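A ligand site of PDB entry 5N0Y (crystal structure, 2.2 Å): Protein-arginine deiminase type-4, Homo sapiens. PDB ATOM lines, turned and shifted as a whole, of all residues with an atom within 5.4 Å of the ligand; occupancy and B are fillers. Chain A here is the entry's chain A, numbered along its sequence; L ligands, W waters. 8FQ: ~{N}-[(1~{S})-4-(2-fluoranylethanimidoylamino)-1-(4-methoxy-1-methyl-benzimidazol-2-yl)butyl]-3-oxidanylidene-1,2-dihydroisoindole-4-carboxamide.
Gln 353 touches the ligand. Gln 356 touches the ligand. OG of Ser 413 touches C1 of the ligand, 3.8 Å away. Gly 415 touches the ligand (CA to N15, 3.8 Å). CG2 of Val 476 touches C30 of the ligand, at 3.5 Å. His 647 touches the ligand. Within 4 Å of the ligand: Gln 353, Trp 354, Gln 356, Asp 357, Arg 381, Ser 413, Gly 415, Val 476, His 478, Asp 480, Arg 646, His 647 and Cys 652.
Water W1 lies within hydrogen-bond range of the side-chain carboxylate (OD2) of Asp 357 (2.7 Å), the guanidinium group (NE) of Arg 379 (2.9 Å) and a nitrogen (N5) of the ligand (2.9 Å). Water W2 lies within hydrogen-bond range of OG of Ser 413 (2.7 Å), O2 of the ligand (3.0 Å) and NE2 of His 478 (3.4 Å). Water W5 lies within hydrogen-bond range of the guanidinium group of Arg 381, an oxygen (O18) of the ligand and the guanidinium group of Arg 379. Water W3 lies within hydrogen-bond range of the backbone carbonyl oxygen of His 647 (2.7 Å) and the side-chain carboxylate of Glu 481 (2.7 Å).
O of Cys 652 sits close to N of Gln 356. The backbone NH of Cys 652 is in hydrogen-bond range of the side-chain amide oxygen of Asn 595 (3.1 Å). The side-chain sulfur of Cys 652 sits at hydrogen-bond distance from the backbone NH of Glu 649 (3.4 Å). OD1 of Asp 357 is in hydrogen-bond range of N of Gly 415 (3.2 Å). The backbone carbonyl oxygen (O) of Asp 480 lies within hydrogen-bond range of the side-chain amide nitrogen (ND2) of Asn 595, 3.2 Å away. A ring nitrogen (NE2) of His 478 lies within hydrogen-bond range of the backbone carbonyl oxygen (O) of Gly 410 (3.2 Å). The backbone NH (N) of His 478 lies within hydrogen-bond range of the side-chain carboxylate (OE2) of Glu 481, 2.9 Å away. The backbone carbonyl oxygen (O) of Gly 410 is in hydrogen-bond range of the side-chain hydroxyl (OG) of Ser 413 (3.3 Å).
The side-chain sulfur (SG) of Cys 652 is bonded to a carbon (C14) of the ligand. The side-chain carboxylate (OD2) of Asp 357 lies within salt-bridge range of a nitrogen (N12) of the ligand (2.7 Å). The backbone carbonyl oxygen of Arg 646 sits at hydrogen-bond distance from a nitrogen (N16) of the ligand (2.8 Å). An oxygen (O22) of the ligand is in hydrogen-bond range of the indole nitrogen (NE1) of Trp 354, at 3.2 Å. An oxygen (O2) of the ligand lies within hydrogen-bond range of the guanidinium group (NH2) of Arg 381, 3.2 Å away. OD2 of Asp 480 is in salt-bridge range of N15 of the ligand (3.2 Å). N15 of the ligand lies within hydrogen-bond range of ND1 of His 478, 3.2 Å away.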
ATOM      1  N   ASP A 351      12.295  13.662   4.593  1.00  0.00           N
ATOM      2  CA  ASP A 351      13.661  13.799   4.006  1.00  0.00           C
ATOM      3  C   ASP A 351      14.600  14.772   4.711  1.00  0.00           C
ATOM      4  O   ASP A 351      15.619  15.171   4.140  1.00  0.00           O
ATOM      5  CB  ASP A 351      13.619  14.199   2.512  1.00  0.00           C
ATOM      6  CG  ASP A 351      12.855  13.211   1.652  1.00  0.00           C
ATOM      7  OD1 ASP A 351      12.738  12.016   2.033  1.00  0.00           O
ATOM      8  OD2 ASP A 351      12.398  13.636   0.559  1.00  0.00           O
ATOM      9  N   GLN A 353      17.261  15.031   7.234  1.00  0.00           N
ATOM     10  CA  GLN A 353      18.205  14.129   7.957  1.00  0.00           C
ATOM     11  C   GLN A 353      18.956  14.823   9.105  1.00  0.00           C
ATOM     12  O   GLN A 353      19.711  14.141   9.842  1.00  0.00           O
ATOM     13  CB  GLN A 353      19.241  13.563   6.997  1.00  0.00           C
ATOM     14  CG  GLN A 353      20.269  14.587   6.521  1.00  0.00           C
ATOM     15  CD  GLN A 353      20.862  14.269   5.181  1.00  0.00           C
ATOM     16  OE1 GLN A 353      20.352  14.724   4.154  1.00  0.00           O
ATOM     17  NE2 GLN A 353      21.950  13.504   5.175  1.00  0.00           N
ATOM     18  N   TRP A 354      18.742  16.144   9.258  1.00  0.00           N
ATOM     19  CA  TRP A 354      19.577  16.981  10.153  1.00  0.00           C
ATOM     20  C   TRP A 354      18.967  17.049  11.551  1.00  0.00           C
ATOM     21  O   TRP A 354      18.360  18.052  11.940  1.00  0.00           O
ATOM     22  CB  TRP A 354      19.802  18.357   9.552  1.00  0.00           C
ATOM     23  CG  TRP A 354      20.272  18.262   8.134  1.00  0.00           C
ATOM     24  CD1 TRP A 354      19.548  18.535   6.999  1.00  0.00           C
ATOM     25  CD2 TRP A 354      21.561  17.786   7.686  1.00  0.00           C
ATOM     26  NE1 TRP A 354      20.323  18.305   5.878  1.00  0.00           N
ATOM     27  CE2 TRP A 354      21.549  17.837   6.269  1.00  0.00           C
ATOM     28  CE3 TRP A 354      22.716  17.356   8.343  1.00  0.00           C
ATOM     29  CZ2 TRP A 354      22.676  17.486   5.511  1.00  0.00           C
ATOM     30  CZ3 TRP A 354      23.830  16.987   7.569  1.00  0.00           C
ATOM     31  CH2 TRP A 354      23.795  17.063   6.175  1.00  0.00           C
ATOM     32  N   GLN A 356      20.303  17.146  14.438  1.00  0.00           N
ATOM     33  CA  GLN A 356      20.961  18.163  15.249  1.00  0.00           C
ATOM     34  C   GLN A 356      20.240  19.494  15.238  1.00  0.00           C
ATOM     35  O   GLN A 356      20.277  20.249  16.202  1.00  0.00           O
ATOM     36  CB  GLN A 356      22.398  18.395  14.752  1.00  0.00           C
ATOM     37  CG  GLN A 356      23.231  19.481  15.482  1.00  0.00           C
ATOM     38  CD  GLN A 356      23.494  19.197  16.950  1.00  0.00           C
ATOM     39  OE1 GLN A 356      23.755  20.096  17.720  1.00  0.00           O
ATOM     40  NE2 GLN A 356      23.452  17.958  17.313  1.00  0.00           N
ATOM     41  N   ASP A 357      19.605  19.800  14.128  1.00  0.00           N
ATOM     42  CA  ASP A 357      19.263  21.179  13.866  1.00  0.00           C
ATOM     43  C   ASP A 357      17.888  21.644  14.368  1.00  0.00           C
ATOM     44  O   ASP A 357      17.698  22.866  14.618  1.00  0.00           O
ATOM     45  CB  ASP A 357      19.453  21.470  12.378  1.00  0.00           C
ATOM     46  CG  ASP A 357      20.944  21.563  11.988  1.00  0.00           C
ATOM     47  OD1 ASP A 357      21.797  21.782  12.916  1.00  0.00           O
ATOM     48  OD2 ASP A 357      21.257  21.408  10.775  1.00  0.00           O
ATOM     49  N   ARG A 379      13.367  26.545  13.224  1.00  0.00           N
ATOM     50  CA  ARG A 379      13.773  26.001  11.927  1.00  0.00           C
ATOM     51  C   ARG A 379      12.580  25.491  11.090  1.00  0.00           C
ATOM     52  O   ARG A 379      12.362  25.951   9.976  1.00  0.00           O
ATOM     53  CB  ARG A 379      14.804  24.875  12.151  1.00  0.00           C
ATOM     54  CG  ARG A 379      15.502  24.403  10.896  1.00  0.00           C
ATOM     55  CD  ARG A 379      16.538  23.381  11.288  1.00  0.00           C
ATOM     56  NE  ARG A 379      17.004  22.559  10.169  1.00  0.00           N
ATOM     57  CZ  ARG A 379      16.601  21.308   9.892  1.00  0.00           C
ATOM     58  NH1 ARG A 379      17.127  20.661   8.864  1.00  0.00           N
ATOM     59  NH2 ARG A 379      15.689  20.684  10.640  1.00  0.00           N
ATOM     60  N   ARG A 381      11.670  22.652   9.394  1.00  0.00           N
ATOM     61  CA  ARG A 381      11.773  21.915   8.143  1.00  0.00           C
ATOM     62  C   ARG A 381      11.082  20.548   8.331  1.00  0.00           C
ATOM     63  O   ARG A 381      10.220  20.398   9.196  1.00  0.00           O
ATOM     64  CB  ARG A 381      13.254  21.829   7.726  1.00  0.00           C
ATOM     65  CG  ARG A 381      13.724  23.129   7.121  1.00  0.00           C
ATOM     66  CD  ARG A 381      15.143  23.028   6.623  1.00  0.00           C
ATOM     67  NE  ARG A 381      15.395  24.174   5.734  1.00  0.00           N
ATOM     68  CZ  ARG A 381      16.388  24.264   4.837  1.00  0.00           C
ATOM     69  NH1 ARG A 381      16.491  25.359   4.075  1.00  0.00           N
ATOM     70  NH2 ARG A 381      17.305  23.298   4.734  1.00  0.00           N
ATOM     71  N   SER A 409      16.661  32.356  10.211  1.00  0.00           N
ATOM     72  CA  SER A 409      17.858  32.175   9.409  1.00  0.00           C
ATOM     73  C   SER A 409      18.486  30.842   9.760  1.00  0.00           C
ATOM     74  O   SER A 409      18.007  30.126  10.656  1.00  0.00           O
ATOM     75  CB  SER A 409      18.840  33.367   9.598  1.00  0.00           C
ATOM     76  OG  SER A 409      19.669  33.240  10.737  1.00  0.00           O
ATOM     77  N   GLY A 410      19.562  30.492   9.065  1.00  0.00           N
ATOM     78  CA  GLY A 410      20.291  29.269   9.380  1.00  0.00           C
ATOM     79  C   GLY A 410      20.832  29.269  10.791  1.00  0.00           C
ATOM     80  O   GLY A 410      20.862  28.241  11.470  1.00  0.00           O
ATOM     81  N   SER A 413      19.193  27.324  13.725  1.00  0.00           N
ATOM     82  CA  SER A 413      19.275  25.863  13.774  1.00  0.00           C
ATOM     83  C   SER A 413      20.219  25.460  14.914  1.00  0.00           C
ATOM     84  O   SER A 413      21.209  26.170  15.194  1.00  0.00           O
ATOM     85  CB  SER A 413      19.789  25.310  12.429  1.00  0.00           C
ATOM     86  OG  SER A 413      18.920  25.632  11.325  1.00  0.00           O
ATOM     87  N   GLY A 415      22.459  23.173  15.689  1.00  0.00           N
ATOM     88  CA  GLY A 415      23.869  22.928  15.595  1.00  0.00           C
ATOM     89  C   GLY A 415      24.624  24.216  15.897  1.00  0.00           C
ATOM     90  O   GLY A 415      25.868  24.184  16.086  1.00  0.00           O
ATOM     91  N   VAL A 476      27.155  27.362   6.344  1.00  0.00           N
ATOM     92  CA  VAL A 476      25.984  26.933   7.117  1.00  0.00           C
ATOM     93  C   VAL A 476      25.815  27.825   8.384  1.00  0.00           C
ATOM     94  O   VAL A 476      24.698  28.166   8.770  1.00  0.00           O
ATOM     95  CB  VAL A 476      26.154  25.414   7.468  1.00  0.00           C
ATOM     96  CG1 VAL A 476      25.278  24.978   8.650  1.00  0.00           C
ATOM     97  CG2 VAL A 476      25.837  24.583   6.227  1.00  0.00           C
ATOM     98  N   HIS A 478      27.470  27.430  11.799  1.00  0.00           N
ATOM     99  CA  HIS A 478      27.159  26.841  13.096  1.00  0.00           C
ATOM    100  C   HIS A 478      28.404  26.630  13.913  1.00  0.00           C
ATOM    101  O   HIS A 478      29.419  26.147  13.395  1.00  0.00           O
ATOM    102  CB  HIS A 478      26.511  25.499  12.882  1.00  0.00           C
ATOM    103  CG  HIS A 478      25.140  25.563  12.331  1.00  0.00           C
ATOM    104  ND1 HIS A 478      24.343  24.451  12.247  1.00  0.00           N
ATOM    105  CD2 HIS A 478      24.425  26.607  11.812  1.00  0.00           C
ATOM    106  CE1 HIS A 478      23.175  24.815  11.725  1.00  0.00           C
ATOM    107  NE2 HIS A 478      23.192  26.105  11.445  1.00  0.00           N
ATOM    108  N   ASP A 480      29.035  24.248  15.886  1.00  0.00           N
ATOM    109  CA  ASP A 480      29.471  22.837  15.834  1.00  0.00           C
ATOM    110  C   ASP A 480      30.378  22.553  14.625  1.00  0.00           C
ATOM    111  O   ASP A 480      31.097  21.570  14.574  1.00  0.00           O
ATOM    112  CB  ASP A 480      28.273  21.838  15.990  1.00  0.00           C
ATOM    113  CG  ASP A 480      27.377  21.675  14.704  1.00  0.00           C
ATOM    114  OD1 ASP A 480      27.506  22.479  13.748  1.00  0.00           O
ATOM    115  OD2 ASP A 480      26.567  20.662  14.623  1.00  0.00           O
ATOM    116  N   GLU A 481      30.404  23.444  13.647  1.00  0.00           N
ATOM    117  CA  GLU A 481      31.311  23.250  12.540  1.00  0.00           C
ATOM    118  C   GLU A 481      32.777  23.540  12.839  1.00  0.00           C
ATOM    119  O   GLU A 481      33.647  23.255  11.999  1.00  0.00           O
ATOM    120  CB  GLU A 481      30.899  24.079  11.356  1.00  0.00           C
ATOM    121  CG  GLU A 481      29.523  23.818  10.834  1.00  0.00           C
ATOM    122  CD  GLU A 481      29.258  24.679   9.620  1.00  0.00           C
ATOM    123  OE1 GLU A 481      29.661  24.247   8.500  1.00  0.00           O
ATOM    124  OE2 GLU A 481      28.652  25.777   9.778  1.00  0.00           O
ATOM    125  N   ASN A 595      33.179  17.848  13.811  1.00  0.00           N
ATOM    126  CA  ASN A 595      31.734  17.683  13.860  1.00  0.00           C
ATOM    127  C   ASN A 595      31.400  16.221  14.172  1.00  0.00           C
ATOM    128  O   ASN A 595      30.834  15.493  13.344  1.00  0.00           O
ATOM    129  CB  ASN A 595      31.162  18.126  12.532  1.00  0.00           C
ATOM    130  CG  ASN A 595      29.702  18.264  12.570  1.00  0.00           C
ATOM    131  OD1 ASN A 595      28.966  17.329  12.172  1.00  0.00           O
ATOM    132  ND2 ASN A 595      29.233  19.389  13.110  1.00  0.00           N
ATOM    133  N   ILE A 645      28.534  15.619   1.487  1.00  0.00           N
ATOM    134  CA  ILE A 645      28.237  16.323   0.214  1.00  0.00           C
ATOM    135  C   ILE A 645      26.959  17.172   0.282  1.00  0.00           C
ATOM    136  O   ILE A 645      26.744  18.019  -0.590  1.00  0.00           O
ATOM    137  CB  ILE A 645      28.209  15.387  -1.033  1.00  0.00           C
ATOM    138  CG1 ILE A 645      27.028  14.380  -0.978  1.00  0.00           C
ATOM    139  CG2 ILE A 645      29.593  14.738  -1.221  1.00  0.00           C
ATOM    140  CD1 ILE A 645      26.741  13.680  -2.297  1.00  0.00           C
ATOM    141  N   ARG A 646      26.112  16.929   1.280  1.00  0.00           N
ATOM    142  CA  ARG A 646      25.083  17.902   1.630  1.00  0.00           C
ATOM    143  C   ARG A 646      25.486  18.866   2.808  1.00  0.00           C
ATOM    144  O   ARG A 646      24.626  19.440   3.502  1.00  0.00           O
ATOM    145  CB  ARG A 646      23.780  17.215   1.931  1.00  0.00           C
ATOM    146  CG  ARG A 646      23.315  16.113   0.971  1.00  0.00           C
ATOM    147  CD  ARG A 646      22.501  15.171   1.829  1.00  0.00           C
ATOM    148  NE  ARG A 646      22.085  13.925   1.218  1.00  0.00           N
ATOM    149  CZ  ARG A 646      20.898  13.697   0.667  1.00  0.00           C
ATOM    150  NH1 ARG A 646      20.001  14.657   0.556  1.00  0.00           N
ATOM    151  NH2 ARG A 646      20.647  12.484   0.204  1.00  0.00           N
ATOM    152  N   HIS A 647      26.796  19.069   2.988  1.00  0.00           N
ATOM    153  CA  HIS A 647      27.336  20.173   3.779  1.00  0.00           C
ATOM    154  C   HIS A 647      27.076  20.009   5.271  1.00  0.00           C
ATOM    155  O   HIS A 647      26.922  21.003   5.974  1.00  0.00           O
ATOM    156  CB  HIS A 647      26.803  21.518   3.267  1.00  0.00           C
ATOM    157  CG  HIS A 647      27.017  21.736   1.808  1.00  0.00           C
ATOM    158  ND1 HIS A 647      26.027  22.215   0.967  1.00  0.00           N
ATOM    159  CD2 HIS A 647      28.107  21.557   1.025  1.00  0.00           C
ATOM    160  CE1 HIS A 647      26.503  22.342  -0.263  1.00  0.00           C
ATOM    161  NE2 HIS A 647      27.763  21.937  -0.249  1.00  0.00           N
ATOM    162  N   GLY A 648      27.044  18.766   5.763  1.00  0.00           N
ATOM    163  CA  GLY A 648      27.081  18.503   7.200  1.00  0.00           C
ATOM    164  C   GLY A 648      27.746  17.181   7.475  1.00  0.00           C
ATOM    165  O   GLY A 648      28.010  16.479   6.543  1.00  0.00           O
ATOM    166  N   GLU A 649      27.981  16.846   8.745  1.00  0.00           N
ATOM    167  CA  GLU A 649      28.621  15.551   9.128  1.00  0.00           C
ATOM    168  C   GLU A 649      27.823  14.750  10.187  1.00  0.00           C
ATOM    169  O   GLU A 649      26.585  14.835  10.259  1.00  0.00           O
ATOM    170  CB  GLU A 649      30.100  15.777   9.563  1.00  0.00           C
ATOM    171  CG  GLU A 649      30.906  16.739   8.700  1.00  0.00           C
ATOM    172  CD  GLU A 649      31.142  16.251   7.264  1.00  0.00           C
ATOM    173  OE1 GLU A 649      31.587  17.071   6.422  1.00  0.00           O
ATOM    174  OE2 GLU A 649      30.935  15.039   7.009  1.00  0.00           O
ATOM    175  N   CYS A 652      25.938  16.817  12.866  1.00  0.00           N
ATOM    176  CA  CYS A 652      24.774  17.423  12.257  1.00  0.00           C
ATOM    177  C   CYS A 652      23.598  16.462  11.975  1.00  0.00           C
ATOM    178  O   CYS A 652      22.445  16.919  11.819  1.00  0.00           O
ATOM    179  CB  CYS A 652      25.198  18.034  10.907  1.00  0.00           C
ATOM    180  SG  CYS A 652      26.664  19.117  10.944  1.00  0.00           S
HETATM  181  C27 8FQ L   1      22.723  20.559  -0.025  1.00  0.00           C
HETATM  182  C33 8FQ L   1      20.664  26.979   4.907  1.00  0.00           C
HETATM  183  C28 8FQ L   1      22.428  20.864   1.305  1.00  0.00           C
HETATM  184  C26 8FQ L   1      22.004  19.572  -0.678  1.00  0.00           C
HETATM  185  C32 8FQ L   1      21.600  26.070   4.470  1.00  0.00           C
HETATM  186  C34 8FQ L   1      19.671  26.617   5.804  1.00  0.00           C
HETATM  187  C20 8FQ L   1      20.699  19.243   1.355  1.00  0.00           C
HETATM  188  C19 8FQ L   1      21.418  20.228   2.022  1.00  0.00           C
HETATM  189  C25 8FQ L   1      21.001  18.937   0.033  1.00  0.00           C
HETATM  190  C4  8FQ L   1      20.499  24.404   5.914  1.00  0.00           C
HETATM  191  C31 8FQ L   1      21.470  24.797   4.999  1.00  0.00           C
HETATM  192  C3  8FQ L   1      19.555  25.335   6.332  1.00  0.00           C
HETATM  193  C6  8FQ L   1      21.647  22.649   5.588  1.00  0.00           C
HETATM  194  C21 8FQ L   1      19.580  18.370   1.788  1.00  0.00           C
HETATM  195  C17 8FQ L   1      21.165  20.638   3.427  1.00  0.00           C
HETATM  196  C13 8FQ L   1      24.787  21.099  11.039  1.00  0.00           C
HETATM  197  C24 8FQ L   1      20.112  17.875  -0.475  1.00  0.00           C
HETATM  198  C14 8FQ L   1      26.217  20.732  10.684  1.00  0.00           C
HETATM  199  C30 8FQ L   1      23.351  23.598   3.900  1.00  0.00           C
HETATM  200  C1  8FQ L   1      17.643  25.809   7.700  1.00  0.00           C
HETATM  201  C10 8FQ L   1      22.962  21.114   7.893  1.00  0.00           C
HETATM  202  C9  8FQ L   1      23.342  21.129   6.443  1.00  0.00           C
HETATM  203  C11 8FQ L   1      24.221  20.926   8.699  1.00  0.00           C
HETATM  204  C7  8FQ L   1      22.107  21.269   5.639  1.00  0.00           C
HETATM  205  N5  8FQ L   1      20.609  23.082   6.278  1.00  0.00           N
HETATM  206  N15 8FQ L   1      24.419  21.219  12.276  1.00  0.00           N
HETATM  207  N29 8FQ L   1      22.194  23.648   4.809  1.00  0.00           N
HETATM  208  N23 8FQ L   1      19.187  17.715   0.644  1.00  0.00           N
HETATM  209  N16 8FQ L   1      22.273  20.738   4.283  1.00  0.00           N
HETATM  210  N12 8FQ L   1      23.888  21.278  10.039  1.00  0.00           N
HETATM  211  O22 8FQ L   1      19.143  18.214   2.923  1.00  0.00           O
HETATM  212  O18 8FQ L   1      19.997  20.894   3.733  1.00  0.00           O
HETATM  213  O2  8FQ L   1      18.603  24.842   7.250  1.00  0.00           O
HETATM  214  O   HOH W   1      19.660  22.678   9.006  1.00  0.00           O
HETATM  215  O   HOH W   2      20.718  25.343   9.298  1.00  0.00           O
HETATM  216  O   HOH W   3      28.172  21.996   8.159  1.00  0.00           O
HETATM  217  O   HOH W   4      22.287  27.094   7.950  1.00  0.00           O
HETATM  218  O   HOH W   5      17.425  20.881   5.642  1.00  0.00           O
HETATM  219  O   HOH W   6      15.676  28.228   8.560  1.00  0.00           O
